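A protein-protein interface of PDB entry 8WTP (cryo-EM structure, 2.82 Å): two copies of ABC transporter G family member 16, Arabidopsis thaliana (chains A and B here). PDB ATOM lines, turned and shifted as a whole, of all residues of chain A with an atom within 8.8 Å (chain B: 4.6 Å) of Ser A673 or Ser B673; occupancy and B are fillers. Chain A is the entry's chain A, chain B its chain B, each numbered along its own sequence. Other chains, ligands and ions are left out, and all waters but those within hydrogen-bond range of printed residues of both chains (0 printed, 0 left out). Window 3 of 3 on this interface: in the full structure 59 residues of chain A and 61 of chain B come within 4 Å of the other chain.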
ATOM      1  N   PHE A 654      -5.374   3.769 -20.800  1.00  0.00           N
ATOM      2  CA  PHE A 654      -6.030   5.020 -21.165  1.00  0.00           C
ATOM      3  C   PHE A 654      -7.462   4.689 -21.562  1.00  0.00           C
ATOM      4  O   PHE A 654      -7.749   4.385 -22.719  1.00  0.00           O
ATOM      5  CB  PHE A 654      -5.280   5.711 -22.295  1.00  0.00           C
ATOM      6  CG  PHE A 654      -3.791   5.598 -22.187  1.00  0.00           C
ATOM      7  CD1 PHE A 654      -3.091   6.365 -21.267  1.00  0.00           C
ATOM      8  CD2 PHE A 654      -3.091   4.728 -23.004  1.00  0.00           C
ATOM      9  CE1 PHE A 654      -1.723   6.266 -21.163  1.00  0.00           C
ATOM     10  CE2 PHE A 654      -1.719   4.623 -22.903  1.00  0.00           C
ATOM     11  CZ  PHE A 654      -1.035   5.396 -21.981  1.00  0.00           C
ATOM     12  N   LEU A 659      -6.781  11.238 -22.037  1.00  0.00           N
ATOM     13  CA  LEU A 659      -6.284  10.067 -22.742  1.00  0.00           C
ATOM     14  C   LEU A 659      -7.279   8.935 -22.520  1.00  0.00           C
ATOM     15  O   LEU A 659      -7.465   8.480 -21.387  1.00  0.00           O
ATOM     16  CB  LEU A 659      -4.904   9.683 -22.231  1.00  0.00           C
ATOM     17  CG  LEU A 659      -3.848  10.762 -22.377  1.00  0.00           C
ATOM     18  CD1 LEU A 659      -2.573  10.224 -21.789  1.00  0.00           C
ATOM     19  CD2 LEU A 659      -3.685  11.138 -23.831  1.00  0.00           C
ATOM     20  N   MET A 666      -3.015   3.675 -32.789  1.00  0.00           N
ATOM     21  CA  MET A 666      -1.881   4.448 -32.303  1.00  0.00           C
ATOM     22  C   MET A 666      -1.589   4.166 -30.833  1.00  0.00           C
ATOM     23  O   MET A 666      -0.486   4.469 -30.363  1.00  0.00           O
ATOM     24  CB  MET A 666      -2.168   5.943 -32.542  1.00  0.00           C
ATOM     25  CG  MET A 666      -1.022   6.949 -32.355  1.00  0.00           C
ATOM     26  SD  MET A 666      -0.829   7.613 -30.688  1.00  0.00           S
ATOM     27  CE  MET A 666      -2.290   8.631 -30.578  1.00  0.00           C
ATOM     28  N   LYS A 667      -2.519   3.500 -30.132  1.00  0.00           N
ATOM     29  CA  LYS A 667      -2.394   3.247 -28.696  1.00  0.00           C
ATOM     30  C   LYS A 667      -1.213   2.343 -28.363  1.00  0.00           C
ATOM     31  O   LYS A 667      -0.688   2.406 -27.246  1.00  0.00           O
ATOM     32  CB  LYS A 667      -3.683   2.622 -28.157  1.00  0.00           C
ATOM     33  CG  LYS A 667      -4.672   3.599 -27.550  1.00  0.00           C
ATOM     34  CD  LYS A 667      -5.997   2.913 -27.270  1.00  0.00           C
ATOM     35  CE  LYS A 667      -6.997   3.862 -26.653  1.00  0.00           C
ATOM     36  NZ  LYS A 667      -6.546   4.298 -25.312  1.00  0.00           N
ATOM     37  N   LEU A 668      -0.784   1.502 -29.311  1.00  0.00           N
ATOM     38  CA  LEU A 668       0.352   0.619 -29.059  1.00  0.00           C
ATOM     39  C   LEU A 668       1.654   1.404 -29.008  1.00  0.00           C
ATOM     40  O   LEU A 668       2.493   1.165 -28.133  1.00  0.00           O
ATOM     41  CB  LEU A 668       0.431  -0.472 -30.126  1.00  0.00           C
ATOM     42  CG  LEU A 668      -0.349  -1.783 -29.962  1.00  0.00           C
ATOM     43  CD1 LEU A 668       0.123  -2.541 -28.732  1.00  0.00           C
ATOM     44  CD2 LEU A 668      -1.852  -1.575 -29.923  1.00  0.00           C
ATOM     45  N   ARG A 669       1.833   2.356 -29.925  1.00  0.00           N
ATOM     46  CA  ARG A 669       2.980   3.253 -29.857  1.00  0.00           C
ATOM     47  C   ARG A 669       2.795   4.328 -28.799  1.00  0.00           C
ATOM     48  O   ARG A 669       3.781   4.931 -28.364  1.00  0.00           O
ATOM     49  CB  ARG A 669       3.247   3.891 -31.224  1.00  0.00           C
ATOM     50  CG  ARG A 669       4.198   3.095 -32.119  1.00  0.00           C
ATOM     51  CD  ARG A 669       3.533   1.892 -32.762  1.00  0.00           C
ATOM     52  NE  ARG A 669       2.475   2.255 -33.697  1.00  0.00           N
ATOM     53  CZ  ARG A 669       1.573   1.396 -34.155  1.00  0.00           C
ATOM     54  NH1 ARG A 669       0.642   1.795 -35.011  1.00  0.00           N
ATOM     55  NH2 ARG A 669       1.601   0.134 -33.749  1.00  0.00           N
ATOM     56  N   LEU A 670       1.554   4.585 -28.382  1.00  0.00           N
ATOM     57  CA  LEU A 670       1.342   5.335 -27.149  1.00  0.00           C
ATOM     58  C   LEU A 670       1.801   4.530 -25.944  1.00  0.00           C
ATOM     59  O   LEU A 670       2.261   5.105 -24.952  1.00  0.00           O
ATOM     60  CB  LEU A 670      -0.131   5.720 -27.016  1.00  0.00           C
ATOM     61  CG  LEU A 670      -0.565   6.569 -25.823  1.00  0.00           C
ATOM     62  CD1 LEU A 670       0.179   7.889 -25.814  1.00  0.00           C
ATOM     63  CD2 LEU A 670      -2.062   6.808 -25.872  1.00  0.00           C
ATOM     64  N   LEU A 671       1.707   3.203 -26.023  1.00  0.00           N
ATOM     65  CA  LEU A 671       2.160   2.316 -24.962  1.00  0.00           C
ATOM     66  C   LEU A 671       3.605   1.870 -25.155  1.00  0.00           C
ATOM     67  O   LEU A 671       4.285   1.557 -24.171  1.00  0.00           O
ATOM     68  CB  LEU A 671       1.234   1.101 -24.885  1.00  0.00           C
ATOM     69  CG  LEU A 671       1.340   0.164 -23.688  1.00  0.00           C
ATOM     70  CD1 LEU A 671       0.977   0.920 -22.429  1.00  0.00           C
ATOM     71  CD2 LEU A 671       0.420  -1.008 -23.889  1.00  0.00           C
ATOM     72  N   ASP A 672       4.093   1.834 -26.400  1.00  0.00           N
ATOM     73  CA  ASP A 672       5.508   1.563 -26.637  1.00  0.00           C
ATOM     74  C   ASP A 672       6.383   2.735 -26.210  1.00  0.00           C
ATOM     75  O   ASP A 672       7.545   2.537 -25.839  1.00  0.00           O
ATOM     76  CB  ASP A 672       5.758   1.250 -28.111  1.00  0.00           C
ATOM     77  CG  ASP A 672       5.347  -0.156 -28.487  1.00  0.00           C
ATOM     78  OD1 ASP A 672       5.072  -0.961 -27.573  1.00  0.00           O
ATOM     79  OD2 ASP A 672       5.300  -0.457 -29.698  1.00  0.00           O
ATOM     80  N   SER A 673       5.848   3.956 -26.270  1.00  0.00           N
ATOM     81  CA  SER A 673       6.591   5.113 -25.791  1.00  0.00           C
ATOM     82  C   SER A 673       6.699   5.113 -24.274  1.00  0.00           C
ATOM     83  O   SER A 673       7.658   5.662 -23.720  1.00  0.00           O
ATOM     84  CB  SER A 673       5.924   6.395 -26.277  1.00  0.00           C
ATOM     85  OG  SER A 673       6.720   7.519 -25.965  1.00  0.00           O
ATOM     86  N   VAL A 674       5.715   4.523 -23.594  1.00  0.00           N
ATOM     87  CA  VAL A 674       5.833   4.270 -22.164  1.00  0.00           C
ATOM     88  C   VAL A 674       6.959   3.286 -21.885  1.00  0.00           C
ATOM     89  O   VAL A 674       7.750   3.472 -20.951  1.00  0.00           O
ATOM     90  CB  VAL A 674       4.491   3.763 -21.612  1.00  0.00           C
ATOM     91  CG1 VAL A 674       4.595   3.541 -20.141  1.00  0.00           C
ATOM     92  CG2 VAL A 674       3.396   4.769 -21.900  1.00  0.00           C
ATOM     93  N   SER A 675       7.060   2.236 -22.704  1.00  0.00           N
ATOM     94  CA  SER A 675       8.103   1.230 -22.542  1.00  0.00           C
ATOM     95  C   SER A 675       9.503   1.788 -22.777  1.00  0.00           C
ATOM     96  O   SER A 675      10.470   1.247 -22.232  1.00  0.00           O
ATOM     97  CB  SER A 675       7.833   0.062 -23.487  1.00  0.00           C
ATOM     98  OG  SER A 675       6.626  -0.596 -23.141  1.00  0.00           O
ATOM     99  N   ARG A 676       9.632   2.862 -23.557  1.00  0.00           N
ATOM    100  CA  ARG A 676      10.901   3.548 -23.749  1.00  0.00           C
ATOM    101  C   ARG A 676      11.134   4.658 -22.732  1.00  0.00           C
ATOM    102  O   ARG A 676      11.941   5.558 -22.987  1.00  0.00           O
ATOM    103  CB  ARG A 676      10.982   4.109 -25.169  1.00  0.00           C
ATOM    104  CG  ARG A 676      11.173   3.045 -26.232  1.00  0.00           C
ATOM    105  CD  ARG A 676      11.355   3.656 -27.605  1.00  0.00           C
ATOM    106  NE  ARG A 676      10.139   4.322 -28.063  1.00  0.00           N
ATOM    107  CZ  ARG A 676       9.158   3.711 -28.720  1.00  0.00           C
ATOM    108  NH1 ARG A 676       9.249   2.418 -28.994  1.00  0.00           N
ATOM    109  NH2 ARG A 676       8.086   4.389 -29.103  1.00  0.00           N
ATOM    110  N   SER A 677      10.451   4.613 -21.589  1.00  0.00           N
ATOM    111  CA  SER A 677      10.602   5.633 -20.558  1.00  0.00           C
ATOM    112  C   SER A 677      10.889   5.076 -19.173  1.00  0.00           C
ATOM    113  O   SER A 677      11.426   5.813 -18.337  1.00  0.00           O
ATOM    114  CB  SER A 677       9.348   6.515 -20.489  1.00  0.00           C
ATOM    115  OG  SER A 677       8.960   6.947 -21.782  1.00  0.00           O
ATOM    116  N   ILE A 678      10.552   3.819 -18.896  1.00  0.00           N
ATOM    117  CA  ILE A 678      10.891   3.190 -17.632  1.00  0.00           C
ATOM    118  C   ILE A 678      11.988   2.140 -17.800  1.00  0.00           C
ATOM    119  O   ILE A 678      12.874   2.040 -16.941  1.00  0.00           O
ATOM    120  CB  ILE A 678       9.631   2.576 -16.971  1.00  0.00           C
ATOM    121  CG1 ILE A 678       8.579   3.648 -16.658  1.00  0.00           C
ATOM    122  CG2 ILE A 678       9.950   1.849 -15.664  1.00  0.00           C
ATOM    123  CD1 ILE A 678       7.470   3.786 -17.679  1.00  0.00           C
ATOM    124  N   GLY A 679      12.010   1.428 -18.922  1.00  0.00           N
ATOM    125  CA  GLY A 679      12.910   0.314 -19.129  1.00  0.00           C
ATOM    126  C   GLY A 679      12.208  -1.016 -19.245  1.00  0.00           C
ATOM    127  O   GLY A 679      12.846  -2.008 -19.615  1.00  0.00           O
ATOM    128  N   MET A 680      10.912  -1.063 -18.949  1.00  0.00           N
ATOM    129  CA  MET A 680      10.108  -2.259 -19.100  1.00  0.00           C
ATOM    130  C   MET A 680       9.555  -2.311 -20.523  1.00  0.00           C
ATOM    131  O   MET A 680       9.830  -1.440 -21.350  1.00  0.00           O
ATOM    132  CB  MET A 680       9.001  -2.274 -18.052  1.00  0.00           C
ATOM    133  CG  MET A 680       9.533  -2.335 -16.628  1.00  0.00           C
ATOM    134  SD  MET A 680       8.242  -2.298 -15.372  1.00  0.00           S
ATOM    135  CE  MET A 680       9.224  -2.251 -13.878  1.00  0.00           C
ATOM    136  N   ILE A 682       5.837  -2.884 -22.315  1.00  0.00           N
ATOM    137  CA  ILE A 682       4.402  -2.994 -22.086  1.00  0.00           C
ATOM    138  C   ILE A 682       3.721  -3.205 -23.430  1.00  0.00           C
ATOM    139  O   ILE A 682       4.063  -2.542 -24.416  1.00  0.00           O
ATOM    140  CB  ILE A 682       3.848  -1.748 -21.372  1.00  0.00           C
ATOM    141  CG1 ILE A 682       4.823  -1.253 -20.301  1.00  0.00           C
ATOM    142  CG2 ILE A 682       2.506  -2.045 -20.746  1.00  0.00           C
ATOM    143  CD1 ILE A 682       5.015  -2.196 -19.128  1.00  0.00           C
ATOM    144  N   ARG B 669       9.030  13.185 -18.784  1.00  0.00           N
ATOM    145  CA  ARG B 669       9.405  12.529 -20.029  1.00  0.00           C
ATOM    146  C   ARG B 669       8.304  11.585 -20.486  1.00  0.00           C
ATOM    147  O   ARG B 669       8.043  11.466 -21.688  1.00  0.00           O
ATOM    148  CB  ARG B 669      10.731  11.783 -19.852  1.00  0.00           C
ATOM    149  CG  ARG B 669      11.192  10.976 -21.059  1.00  0.00           C
ATOM    150  CD  ARG B 669      11.622  11.881 -22.204  1.00  0.00           C
ATOM    151  NE  ARG B 669      10.588  12.007 -23.229  1.00  0.00           N
ATOM    152  CZ  ARG B 669      10.414  13.087 -23.984  1.00  0.00           C
ATOM    153  NH1 ARG B 669       9.449  13.118 -24.894  1.00  0.00           N
ATOM    154  NH2 ARG B 669      11.202  14.140 -23.828  1.00  0.00           N
ATOM    155  N   LEU B 670       7.623  10.947 -19.531  1.00  0.00           N
ATOM    156  CA  LEU B 670       6.452  10.137 -19.844  1.00  0.00           C
ATOM    157  C   LEU B 670       5.290  10.998 -20.319  1.00  0.00           C
ATOM    158  O   LEU B 670       4.457  10.538 -21.106  1.00  0.00           O
ATOM    159  CB  LEU B 670       6.055   9.329 -18.612  1.00  0.00           C
ATOM    160  CG  LEU B 670       4.911   8.330 -18.664  1.00  0.00           C
ATOM    161  CD1 LEU B 670       5.218   7.238 -19.663  1.00  0.00           C
ATOM    162  CD2 LEU B 670       4.714   7.758 -17.279  1.00  0.00           C
ATOM    163  N   LEU B 671       5.223  12.249 -19.864  1.00  0.00           N
ATOM    164  CA  LEU B 671       4.137  13.142 -20.243  1.00  0.00           C
ATOM    165  C   LEU B 671       4.435  13.923 -21.516  1.00  0.00           C
ATOM    166  O   LEU B 671       3.517  14.188 -22.298  1.00  0.00           O
ATOM    167  CB  LEU B 671       3.837  14.113 -19.101  1.00  0.00           C
ATOM    168  CG  LEU B 671       2.554  14.925 -19.218  1.00  0.00           C
ATOM    169  CD1 LEU B 671       1.378  13.975 -19.189  1.00  0.00           C
ATOM    170  CD2 LEU B 671       2.466  15.921 -18.092  1.00  0.00           C
ATOM    171  N   ASP B 672       5.696  14.302 -21.744  1.00  0.00           N
ATOM    172  CA  ASP B 672       6.063  14.943 -23.002  1.00  0.00           C
ATOM    173  C   ASP B 672       6.043  13.971 -24.170  1.00  0.00           C
ATOM    174  O   ASP B 672       5.857  14.395 -25.314  1.00  0.00           O
ATOM    175  CB  ASP B 672       7.449  15.576 -22.894  1.00  0.00           C
ATOM    176  CG  ASP B 672       7.408  16.969 -22.318  1.00  0.00           C
ATOM    177  OD1 ASP B 672       6.296  17.463 -22.031  1.00  0.00           O
ATOM    178  OD2 ASP B 672       8.488  17.576 -22.148  1.00  0.00           O
ATOM    179  N   SER B 673       6.237  12.680 -23.904  1.00  0.00           N
ATOM    180  CA  SER B 673       6.151  11.680 -24.956  1.00  0.00           C
ATOM    181  C   SER B 673       4.718  11.426 -25.392  1.00  0.00           C
ATOM    182  O   SER B 673       4.490  11.067 -26.552  1.00  0.00           O
ATOM    183  CB  SER B 673       6.794  10.383 -24.484  1.00  0.00           C
ATOM    184  OG  SER B 673       6.080   9.833 -23.393  1.00  0.00           O
ATOM    185  N   VAL B 674       3.754  11.586 -24.484  1.00  0.00           N
ATOM    186  CA  VAL B 674       2.350  11.529 -24.871  1.00  0.00           C
ATOM    187  C   VAL B 674       2.003  12.712 -25.767  1.00  0.00           C
ATOM    188  O   VAL B 674       1.264  12.572 -26.752  1.00  0.00           O
ATOM    189  CB  VAL B 674       1.465  11.474 -23.612  1.00  0.00           C
ATOM    190  CG1 VAL B 674       0.011  11.606 -23.970  1.00  0.00           C
ATOM    191  CG2 VAL B 674       1.691  10.171 -22.866  1.00  0.00           C
ATOM    192  N   SER B 675       2.586  13.880 -25.478  1.00  0.00           N
ATOM    193  CA  SER B 675       2.420  15.055 -26.330  1.00  0.00           C
ATOM    194  C   SER B 675       3.022  14.850 -27.716  1.00  0.00           C
ATOM    195  O   SER B 675       2.602  15.506 -28.676  1.00  0.00           O
ATOM    196  CB  SER B 675       3.052  16.272 -25.660  1.00  0.00           C
ATOM    197  OG  SER B 675       2.383  16.592 -24.456  1.00  0.00           O
ATOM    198  N   ARG B 676       3.994  13.941 -27.841  1.00  0.00           N
ATOM    199  CA  ARG B 676       4.602  13.588 -29.116  1.00  0.00           C
ATOM    200  C   ARG B 676       3.816  12.526 -29.875  1.00  0.00           C
ATOM    201  O   ARG B 676       4.349  11.929 -30.820  1.00  0.00           O
ATOM    202  CB  ARG B 676       6.032  13.101 -28.886  1.00  0.00           C
ATOM    203  CG  ARG B 676       7.115  14.148 -29.059  1.00  0.00           C
ATOM    204  CD  ARG B 676       8.536  13.560 -29.072  1.00  0.00           C
ATOM    205  NE  ARG B 676       8.853  12.677 -27.946  1.00  0.00           N
ATOM    206  CZ  ARG B 676       8.828  11.346 -27.990  1.00  0.00           C
ATOM    207  NH1 ARG B 676       8.495  10.724 -29.111  1.00  0.00           N
ATOM    208  NH2 ARG B 676       9.135  10.636 -26.913  1.00  0.00           N
ATOM    209  N   SER B 677       2.563  12.268 -29.493  1.00  0.00           N
ATOM    210  CA  SER B 677       1.779  11.205 -30.105  1.00  0.00           C
ATOM    211  C   SER B 677       0.415  11.642 -30.616  1.00  0.00           C
ATOM    212  O   SER B 677      -0.110  11.005 -31.531  1.00  0.00           O
ATOM    213  CB  SER B 677       1.582  10.048 -29.114  1.00  0.00           C
ATOM    214  OG  SER B 677       2.819   9.644 -28.550  1.00  0.00           O
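Ser A673 touches its own counterpart, Ser B673. Val A674 touches Leu B670, but with the chains exchanged Leu A670 does not touch Val B674 (4.02 Å). Positions printed for both chains: 669, 670, 671, 672, 673, 674, 675, 676 and 677. Of the 4 pairs that touch across the chains among the printed residues, 1 has its exchanged pair printed and touching as well.
SD of Met A666 sits close to O of Ser B677 (3.6 Å).
Among the printed residues, merely in contact across the chains: Ser A673 with Ser B673, Leu A659 with Val B674 and Val A674 with Leu B670.
Hydrophobic or aromatic side chains of chain A that line the printed part of chain B: Leu A659, Met A666 and Val A674. Of the 9 printed residues of chain B, 4 touch a printed residue of chain A. Printed residues of chain B that touch a printed residue of chain A: Leu B670, Ser B673, Val B674 and Ser B677. Hydrophobic or aromatic side chains of chain B that line the printed part of chain A: Leu B670 and Val B674. Among the printed residues, 4 pairs touch across the chains. Among the printed residues, no Asp or Glu carboxylate lies within 4 Å of a Lys or Arg side-chain nitrogen of the other chain.
The backbone carbonyl oxygen of Ser A673 lies within hydrogen-bond range of the side-chain hydroxyl of Ser A677 (2.7 Å). The backbone carbonyl oxygen (O) of Arg B669 sits at hydrogen-bond distance from the side-chain hydroxyl (OG) of Ser B673 (3.1 Å). The backbone carbonyl oxygen (O) of Leu B670 is in hydrogen-bond range of the side-chain hydroxyl (OG) of Ser B673 (2.9 Å). The side-chain hydroxyl (OG) of Ser B677 lies within hydrogen-bond range of the backbone carbonyl oxygen (O) of Ser B673 (3.0 Å).
Of the printed residues of chain B, Met A666 touches Ser B677 (3.4 Å). Of chain B, only Ser B673 comes within 4 Å of Ser A673. Of the printed residues of chain B, Val A674 touches Leu B670. Of the printed residues of chain A, Leu B670 touches Val A674. Printed residues of chain A within 4 Å of Ser B673: Ser A673. Printed residues of chain A within 4 Å of Val B674: Leu A659. Printed residues of chain A within 4 Å of Ser B677: Met A666 (3.4 Å). The nearest residue of chain A that does not touch Ser B673 is Ser A677 (4.4 Å). The nearest printed residue of chain B that does not touch Val A674 is Ser B673 (5.3 Å).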
